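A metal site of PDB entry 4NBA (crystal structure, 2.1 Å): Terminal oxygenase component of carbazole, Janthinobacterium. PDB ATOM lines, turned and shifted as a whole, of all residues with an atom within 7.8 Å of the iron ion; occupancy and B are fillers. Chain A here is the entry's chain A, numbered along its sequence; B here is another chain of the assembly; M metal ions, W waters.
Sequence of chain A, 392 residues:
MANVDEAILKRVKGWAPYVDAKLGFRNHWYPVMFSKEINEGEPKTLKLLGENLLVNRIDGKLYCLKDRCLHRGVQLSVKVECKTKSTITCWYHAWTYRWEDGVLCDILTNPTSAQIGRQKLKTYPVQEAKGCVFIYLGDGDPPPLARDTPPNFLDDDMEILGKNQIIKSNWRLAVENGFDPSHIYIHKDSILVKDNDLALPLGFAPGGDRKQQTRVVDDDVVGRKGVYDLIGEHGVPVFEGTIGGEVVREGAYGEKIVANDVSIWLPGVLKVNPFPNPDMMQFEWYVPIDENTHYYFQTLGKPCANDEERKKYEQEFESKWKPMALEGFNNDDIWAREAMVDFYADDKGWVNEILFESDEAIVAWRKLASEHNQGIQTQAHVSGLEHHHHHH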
ATOM      1  N   ASN A 177     -17.607  15.702  20.864  1.00  0.00           N
ATOM      2  CA  ASN A 177     -18.386  14.725  20.092  1.00  0.00           C
ATOM      3  C   ASN A 177     -18.050  13.320  20.607  1.00  0.00           C
ATOM      4  O   ASN A 177     -18.944  12.509  20.854  1.00  0.00           O
ATOM      5  CB  ASN A 177     -18.039  14.796  18.603  1.00  0.00           C
ATOM      6  CG  ASN A 177     -18.722  13.706  17.798  1.00  0.00           C
ATOM      7  OD1 ASN A 177     -19.926  13.765  17.547  1.00  0.00           O
ATOM      8  ND2 ASN A 177     -17.967  12.687  17.423  1.00  0.00           N
ATOM      9  N   GLY A 178     -16.764  13.049  20.798  1.00  0.00           N
ATOM     10  CA  GLY A 178     -16.354  11.745  21.271  1.00  0.00           C
ATOM     11  C   GLY A 178     -16.896  11.337  22.635  1.00  0.00           C
ATOM     12  O   GLY A 178     -17.229  10.172  22.861  1.00  0.00           O
ATOM     13  N   PHE A 179     -16.994  12.303  23.546  1.00  0.00           N
ATOM     14  CA  PHE A 179     -17.482  12.036  24.897  1.00  0.00           C
ATOM     15  C   PHE A 179     -18.991  12.268  25.054  1.00  0.00           C
ATOM     16  O   PHE A 179     -19.565  12.001  26.107  1.00  0.00           O
ATOM     17  CB  PHE A 179     -16.688  12.909  25.882  1.00  0.00           C
ATOM     18  CG  PHE A 179     -16.887  12.530  27.327  1.00  0.00           C
ATOM     19  CD1 PHE A 179     -16.631  11.240  27.767  1.00  0.00           C
ATOM     20  CD2 PHE A 179     -17.301  13.485  28.253  1.00  0.00           C
ATOM     21  CE1 PHE A 179     -16.791  10.886  29.116  1.00  0.00           C
ATOM     22  CE2 PHE A 179     -17.454  13.154  29.606  1.00  0.00           C
ATOM     23  CZ  PHE A 179     -17.204  11.850  30.037  1.00  0.00           C
ATOM     24  N   ASP A 180     -19.632  12.739  23.982  1.00  0.00           N
ATOM     25  CA  ASP A 180     -21.068  13.048  23.955  1.00  0.00           C
ATOM     26  C   ASP A 180     -21.916  11.774  24.071  1.00  0.00           C
ATOM     27  O   ASP A 180     -21.997  10.987  23.131  1.00  0.00           O
ATOM     28  CB  ASP A 180     -21.377  13.761  22.625  1.00  0.00           C
ATOM     29  CG  ASP A 180     -22.786  14.317  22.560  1.00  0.00           C
ATOM     30  OD1 ASP A 180     -23.724  13.693  23.113  1.00  0.00           O
ATOM     31  OD2 ASP A 180     -22.958  15.390  21.933  1.00  0.00           O
ATOM     32  N   HIS A 183     -24.524  11.351  21.177  1.00  0.00           N
ATOM     33  CA  HIS A 183     -24.118  11.352  19.777  1.00  0.00           C
ATOM     34  C   HIS A 183     -24.181   9.954  19.168  1.00  0.00           C
ATOM     35  O   HIS A 183     -24.074   9.798  17.956  1.00  0.00           O
ATOM     36  CB  HIS A 183     -22.713  11.953  19.604  1.00  0.00           C
ATOM     37  CG  HIS A 183     -21.602  10.946  19.641  1.00  0.00           C
ATOM     38  ND1 HIS A 183     -21.131  10.394  20.803  1.00  0.00           N
ATOM     39  CD2 HIS A 183     -20.853  10.417  18.637  1.00  0.00           C
ATOM     40  CE1 HIS A 183     -20.138   9.569  20.534  1.00  0.00           C
ATOM     41  NE2 HIS A 183     -19.954   9.567  19.225  1.00  0.00           N
ATOM     42  N   ILE A 184     -24.345   8.952  20.023  1.00  0.00           N
ATOM     43  CA  ILE A 184     -24.435   7.563  19.588  1.00  0.00           C
ATOM     44  C   ILE A 184     -25.493   7.421  18.474  1.00  0.00           C
ATOM     45  O   ILE A 184     -25.444   6.492  17.668  1.00  0.00           O
ATOM     46  CB  ILE A 184     -24.781   6.653  20.802  1.00  0.00           C
ATOM     47  CG1 ILE A 184     -24.543   5.180  20.466  1.00  0.00           C
ATOM     48  CG2 ILE A 184     -26.230   6.865  21.226  1.00  0.00           C
ATOM     49  CD1 ILE A 184     -24.768   4.254  21.670  1.00  0.00           C
ATOM     50  N   TYR A 185     -26.437   8.359  18.433  1.00  0.00           N
ATOM     51  CA  TYR A 185     -27.496   8.359  17.429  1.00  0.00           C
ATOM     52  C   TYR A 185     -26.939   8.385  16.000  1.00  0.00           C
ATOM     53  O   TYR A 185     -27.539   7.810  15.084  1.00  0.00           O
ATOM     54  CB  TYR A 185     -28.427   9.562  17.644  1.00  0.00           C
ATOM     55  CG  TYR A 185     -29.624   9.603  16.718  1.00  0.00           C
ATOM     56  CD1 TYR A 185     -30.731   8.767  16.918  1.00  0.00           C
ATOM     57  CD2 TYR A 185     -29.649  10.471  15.621  1.00  0.00           C
ATOM     58  CE1 TYR A 185     -31.826   8.788  16.038  1.00  0.00           C
ATOM     59  CE2 TYR A 185     -30.742  10.501  14.737  1.00  0.00           C
ATOM     60  CZ  TYR A 185     -31.820   9.653  14.949  1.00  0.00           C
ATOM     61  OH  TYR A 185     -32.887   9.684  14.079  1.00  0.00           O
ATOM     62  N   ILE A 186     -25.794   9.043  15.795  1.00  0.00           N
ATOM     63  CA  ILE A 186     -25.213   9.131  14.461  1.00  0.00           C
ATOM     64  C   ILE A 186     -24.595   7.829  13.976  1.00  0.00           C
ATOM     65  O   ILE A 186     -24.238   7.701  12.805  1.00  0.00           O
ATOM     66  CB  ILE A 186     -24.115  10.225  14.350  1.00  0.00           C
ATOM     67  CG1 ILE A 186     -22.850   9.773  15.077  1.00  0.00           C
ATOM     68  CG2 ILE A 186     -24.631  11.558  14.916  1.00  0.00           C
ATOM     69  CD1 ILE A 186     -21.672  10.730  14.899  1.00  0.00           C
ATOM     70  N   HIS A 187     -24.446   6.858  14.881  1.00  0.00           N
ATOM     71  CA  HIS A 187     -23.850   5.568  14.558  1.00  0.00           C
ATOM     72  C   HIS A 187     -24.890   4.463  14.358  1.00  0.00           C
ATOM     73  O   HIS A 187     -24.527   3.305  14.172  1.00  0.00           O
ATOM     74  CB  HIS A 187     -22.907   5.140  15.679  1.00  0.00           C
ATOM     75  CG  HIS A 187     -21.719   6.032  15.844  1.00  0.00           C
ATOM     76  ND1 HIS A 187     -20.763   6.191  14.859  1.00  0.00           N
ATOM     77  CD2 HIS A 187     -21.313   6.803  16.881  1.00  0.00           C
ATOM     78  CE1 HIS A 187     -19.838   7.029  15.278  1.00  0.00           C
ATOM     79  NE2 HIS A 187     -20.150   7.421  16.503  1.00  0.00           N
ATOM     80  N   LEU A 270      -9.798  10.076  24.562  1.00  0.00           N
ATOM     81  CA  LEU A 270     -10.942   9.258  24.951  1.00  0.00           C
ATOM     82  C   LEU A 270     -10.609   7.774  25.108  1.00  0.00           C
ATOM     83  O   LEU A 270      -9.810   7.237  24.346  1.00  0.00           O
ATOM     84  CB  LEU A 270     -12.057   9.407  23.906  1.00  0.00           C
ATOM     85  CG  LEU A 270     -13.440   8.813  24.245  1.00  0.00           C
ATOM     86  CD1 LEU A 270     -14.200   9.782  25.153  1.00  0.00           C
ATOM     87  CD2 LEU A 270     -14.227   8.562  22.964  1.00  0.00           C
ATOM     88  N   PHE A 275     -14.238  -1.878  23.317  1.00  0.00           N
ATOM     89  CA  PHE A 275     -14.639  -1.444  21.980  1.00  0.00           C
ATOM     90  C   PHE A 275     -13.514  -1.735  20.993  1.00  0.00           C
ATOM     91  O   PHE A 275     -12.344  -1.595  21.342  1.00  0.00           O
ATOM     92  CB  PHE A 275     -14.943   0.050  21.977  1.00  0.00           C
ATOM     93  CG  PHE A 275     -15.818   0.499  20.833  1.00  0.00           C
ATOM     94  CD1 PHE A 275     -17.199   0.343  20.889  1.00  0.00           C
ATOM     95  CD2 PHE A 275     -15.245   1.058  19.685  1.00  0.00           C
ATOM     96  CE1 PHE A 275     -18.003   0.740  19.830  1.00  0.00           C
ATOM     97  CE2 PHE A 275     -16.051   1.459  18.610  1.00  0.00           C
ATOM     98  CZ  PHE A 275     -17.431   1.299  18.682  1.00  0.00           C
ATOM     99  N   GLU A 284      -8.376   7.158  21.818  1.00  0.00           N
ATOM    100  CA  GLU A 284      -8.193   8.103  20.708  1.00  0.00           C
ATOM    101  C   GLU A 284      -7.965   9.540  21.158  1.00  0.00           C
ATOM    102  O   GLU A 284      -8.676  10.067  22.030  1.00  0.00           O
ATOM    103  CB  GLU A 284      -9.376   8.049  19.729  1.00  0.00           C
ATOM    104  CG  GLU A 284     -10.757   8.225  20.344  1.00  0.00           C
ATOM    105  CD  GLU A 284     -11.847   8.200  19.273  1.00  0.00           C
ATOM    106  OE1 GLU A 284     -11.758   7.350  18.366  1.00  0.00           O
ATOM    107  OE2 GLU A 284     -12.776   9.030  19.343  1.00  0.00           O
ATOM    108  N   TYR A 286      -7.366  13.717  20.168  1.00  0.00           N
ATOM    109  CA  TYR A 286      -7.821  14.762  19.247  1.00  0.00           C
ATOM    110  C   TYR A 286      -6.755  15.835  19.507  1.00  0.00           C
ATOM    111  O   TYR A 286      -6.909  16.685  20.388  1.00  0.00           O
ATOM    112  CB  TYR A 286      -9.214  15.249  19.660  1.00  0.00           C
ATOM    113  CG  TYR A 286     -10.176  14.129  19.984  1.00  0.00           C
ATOM    114  CD1 TYR A 286     -10.749  13.351  18.982  1.00  0.00           C
ATOM    115  CD2 TYR A 286     -10.499  13.820  21.314  1.00  0.00           C
ATOM    116  CE1 TYR A 286     -11.613  12.293  19.287  1.00  0.00           C
ATOM    117  CE2 TYR A 286     -11.373  12.771  21.635  1.00  0.00           C
ATOM    118  CZ  TYR A 286     -11.926  12.025  20.613  1.00  0.00           C
ATOM    119  OH  TYR A 286     -12.798  10.998  20.909  1.00  0.00           O
ATOM    120  N   TYR A 296      -6.483  13.169  14.401  1.00  0.00           N
ATOM    121  CA  TYR A 296      -7.423  12.219  14.976  1.00  0.00           C
ATOM    122  C   TYR A 296      -6.546  10.961  15.073  1.00  0.00           C
ATOM    123  O   TYR A 296      -6.450  10.169  14.124  1.00  0.00           O
ATOM    124  CB  TYR A 296      -8.631  12.009  14.060  1.00  0.00           C
ATOM    125  CG  TYR A 296      -9.642  10.994  14.564  1.00  0.00           C
ATOM    126  CD1 TYR A 296      -9.833  10.779  15.932  1.00  0.00           C
ATOM    127  CD2 TYR A 296     -10.404  10.238  13.673  1.00  0.00           C
ATOM    128  CE1 TYR A 296     -10.749   9.831  16.402  1.00  0.00           C
ATOM    129  CE2 TYR A 296     -11.325   9.285  14.131  1.00  0.00           C
ATOM    130  CZ  TYR A 296     -11.481   9.085  15.496  1.00  0.00           C
ATOM    131  OH  TYR A 296     -12.342   8.108  15.951  1.00  0.00           O
ATOM    132  N   PHE A 329     -16.950   2.808  11.613  1.00  0.00           N
ATOM    133  CA  PHE A 329     -17.720   3.375  12.713  1.00  0.00           C
ATOM    134  C   PHE A 329     -17.422   4.854  12.946  1.00  0.00           C
ATOM    135  O   PHE A 329     -18.330   5.687  12.936  1.00  0.00           O
ATOM    136  CB  PHE A 329     -17.427   2.590  13.998  1.00  0.00           C
ATOM    137  CG  PHE A 329     -18.318   2.960  15.154  1.00  0.00           C
ATOM    138  CD1 PHE A 329     -19.586   2.400  15.280  1.00  0.00           C
ATOM    139  CD2 PHE A 329     -17.870   3.834  16.142  1.00  0.00           C
ATOM    140  CE1 PHE A 329     -20.393   2.692  16.375  1.00  0.00           C
ATOM    141  CE2 PHE A 329     -18.662   4.140  17.251  1.00  0.00           C
ATOM    142  CZ  PHE A 329     -19.920   3.572  17.362  1.00  0.00           C
ATOM    143  N   ASN A 330     -16.145   5.182  13.143  1.00  0.00           N
ATOM    144  CA  ASN A 330     -15.739   6.560  13.421  1.00  0.00           C
ATOM    145  C   ASN A 330     -15.791   7.577  12.273  1.00  0.00           C
ATOM    146  O   ASN A 330     -15.710   8.767  12.520  1.00  0.00           O
ATOM    147  CB  ASN A 330     -14.347   6.554  14.051  1.00  0.00           C
ATOM    148  CG  ASN A 330     -14.331   5.869  15.412  1.00  0.00           C
ATOM    149  OD1 ASN A 330     -13.496   4.995  15.663  1.00  0.00           O
ATOM    150  ND2 ASN A 330     -15.245   6.261  16.295  1.00  0.00           N
ATOM    151  N   ASN A 331     -15.906   7.132  11.021  1.00  0.00           N
ATOM    152  CA  ASN A 331     -15.967   8.102   9.935  1.00  0.00           C
ATOM    153  C   ASN A 331     -17.153   9.049  10.124  1.00  0.00           C
ATOM    154  O   ASN A 331     -17.088  10.223   9.760  1.00  0.00           O
ATOM    155  CB  ASN A 331     -16.058   7.416   8.566  1.00  0.00           C
ATOM    156  CG  ASN A 331     -14.698   7.048   8.011  1.00  0.00           C
ATOM    157  OD1 ASN A 331     -13.661   7.439   8.551  1.00  0.00           O
ATOM    158  ND2 ASN A 331     -14.689   6.309   6.901  1.00  0.00           N
ATOM    159  N   ASP A 332     -18.250   8.557  10.701  1.00  0.00           N
ATOM    160  CA  ASP A 332     -19.394   9.426  10.907  1.00  0.00           C
ATOM    161  C   ASP A 332     -19.066  10.537  11.920  1.00  0.00           C
ATOM    162  O   ASP A 332     -19.650  11.604  11.873  1.00  0.00           O
ATOM    163  CB  ASP A 332     -20.618   8.638  11.375  1.00  0.00           C
ATOM    164  CG  ASP A 332     -21.326   7.943  10.233  1.00  0.00           C
ATOM    165  OD1 ASP A 332     -21.490   8.572   9.168  1.00  0.00           O
ATOM    166  OD2 ASP A 332     -21.722   6.768  10.388  1.00  0.00           O
ATOM    167  N   ASP A 333     -18.125  10.263  12.819  1.00  0.00           N
ATOM    168  CA  ASP A 333     -17.709  11.256  13.809  1.00  0.00           C
ATOM    169  C   ASP A 333     -16.973  12.385  13.126  1.00  0.00           C
ATOM    170  O   ASP A 333     -17.077  13.549  13.527  1.00  0.00           O
ATOM    171  CB  ASP A 333     -16.776  10.646  14.848  1.00  0.00           C
ATOM    172  CG  ASP A 333     -17.474   9.650  15.736  1.00  0.00           C
ATOM    173  OD1 ASP A 333     -18.498  10.023  16.343  1.00  0.00           O
ATOM    174  OD2 ASP A 333     -16.989   8.499  15.826  1.00  0.00           O
ATOM    175  N   ILE A 334     -16.209  12.053  12.094  1.00  0.00           N
ATOM    176  CA  ILE A 334     -15.457  13.061  11.374  1.00  0.00           C
ATOM    177  C   ILE A 334     -16.363  14.150  10.812  1.00  0.00           C
ATOM    178  O   ILE A 334     -16.135  15.334  11.084  1.00  0.00           O
ATOM    179  CB  ILE A 334     -14.597  12.439  10.243  1.00  0.00           C
ATOM    180  CG1 ILE A 334     -13.514  11.553  10.856  1.00  0.00           C
ATOM    181  CG2 ILE A 334     -13.965  13.535   9.401  1.00  0.00           C
ATOM    182  CD1 ILE A 334     -12.712  10.735   9.832  1.00  0.00           C
ATOM    183  N   ALA A 336     -19.388  14.764  11.657  1.00  0.00           N
ATOM    184  CA  ALA A 336     -20.203  15.319  12.737  1.00  0.00           C
ATOM    185  C   ALA A 336     -19.416  16.510  13.323  1.00  0.00           C
ATOM    186  O   ALA A 336     -19.993  17.570  13.596  1.00  0.00           O
ATOM    187  CB  ALA A 336     -20.449  14.267  13.807  1.00  0.00           C
ATOM    188  N   ARG A 337     -18.110  16.311  13.508  1.00  0.00           N
ATOM    189  CA  ARG A 337     -17.235  17.357  14.036  1.00  0.00           C
ATOM    190  C   ARG A 337     -17.234  18.554  13.101  1.00  0.00           C
ATOM    191  O   ARG A 337     -17.381  19.689  13.519  1.00  0.00           O
ATOM    192  CB  ARG A 337     -15.795  16.867  14.160  1.00  0.00           C
ATOM    193  CG  ARG A 337     -15.556  15.819  15.202  1.00  0.00           C
ATOM    194  CD  ARG A 337     -14.143  15.280  15.091  1.00  0.00           C
ATOM    195  NE  ARG A 337     -14.099  13.895  15.552  1.00  0.00           N
ATOM    196  CZ  ARG A 337     -13.085  13.065  15.350  1.00  0.00           C
ATOM    197  NH1 ARG A 337     -12.006  13.477  14.691  1.00  0.00           N
ATOM    198  NH2 ARG A 337     -13.163  11.807  15.768  1.00  0.00           N
ATOM    199  N   TYR B  92     -27.971  14.646  14.333  1.00  0.00           N
ATOM    200  CA  TYR B  92     -26.996  14.554  15.418  1.00  0.00           C
ATOM    201  C   TYR B  92     -27.487  13.905  16.719  1.00  0.00           C
ATOM    202  O   TYR B  92     -27.028  12.828  17.075  1.00  0.00           O
ATOM    203  CB  TYR B  92     -26.430  15.945  15.717  1.00  0.00           C
ATOM    204  CG  TYR B  92     -25.006  15.964  16.222  1.00  0.00           C
ATOM    205  CD1 TYR B  92     -24.345  14.780  16.578  1.00  0.00           C
ATOM    206  CD2 TYR B  92     -24.319  17.176  16.385  1.00  0.00           C
ATOM    207  CE1 TYR B  92     -23.034  14.798  17.082  1.00  0.00           C
ATOM    208  CE2 TYR B  92     -23.019  17.207  16.888  1.00  0.00           C
ATOM    209  CZ  TYR B  92     -22.376  16.022  17.234  1.00  0.00           C
ATOM    210  OH  TYR B  92     -21.106  16.074  17.746  1.00  0.00           O
HETATM  211 FE    FE M   1     -18.900   8.651  17.717  1.00  0.00          FE
HETATM  212  O   HOH W   1     -17.678   7.644  18.796  1.00  0.00           O
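The side-chain carboxylate of Asp 333 sits close to the side-chain amide nitrogen of Asn 177. The side-chain carboxylate of Asp 333 lies within hydrogen-bond range of the side-chain amide nitrogen of Asn 330, at 2.9 Å. ND1 of His 183 sits at hydrogen-bond distance from O of Asn 177. A ring nitrogen (ND1) of His 183 sits at hydrogen-bond distance from the backbone carbonyl oxygen (O) of Asp 180. A ring nitrogen (ND1) of His 187 sits close to the backbone carbonyl oxygen (O) of Phe 329 (3.1 Å).
Of the 23 residues printed, 3 come within 4 Å of the iron ion. The nearest printed residue that does not touch the iron ion is Asn 177 (4.2 Å).
Water W1 binds the iron ion (1.9 Å). OD1 of Asp 333 binds the iron ion, at 2.0 Å. A ring nitrogen (NE2) of His 183 binds the iron ion (2.1 Å). NE2 of His 187 binds the iron ion (2.1 Å). Slightly farther from the iron ion lies OD2 of Asp 333 (2.7 Å).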
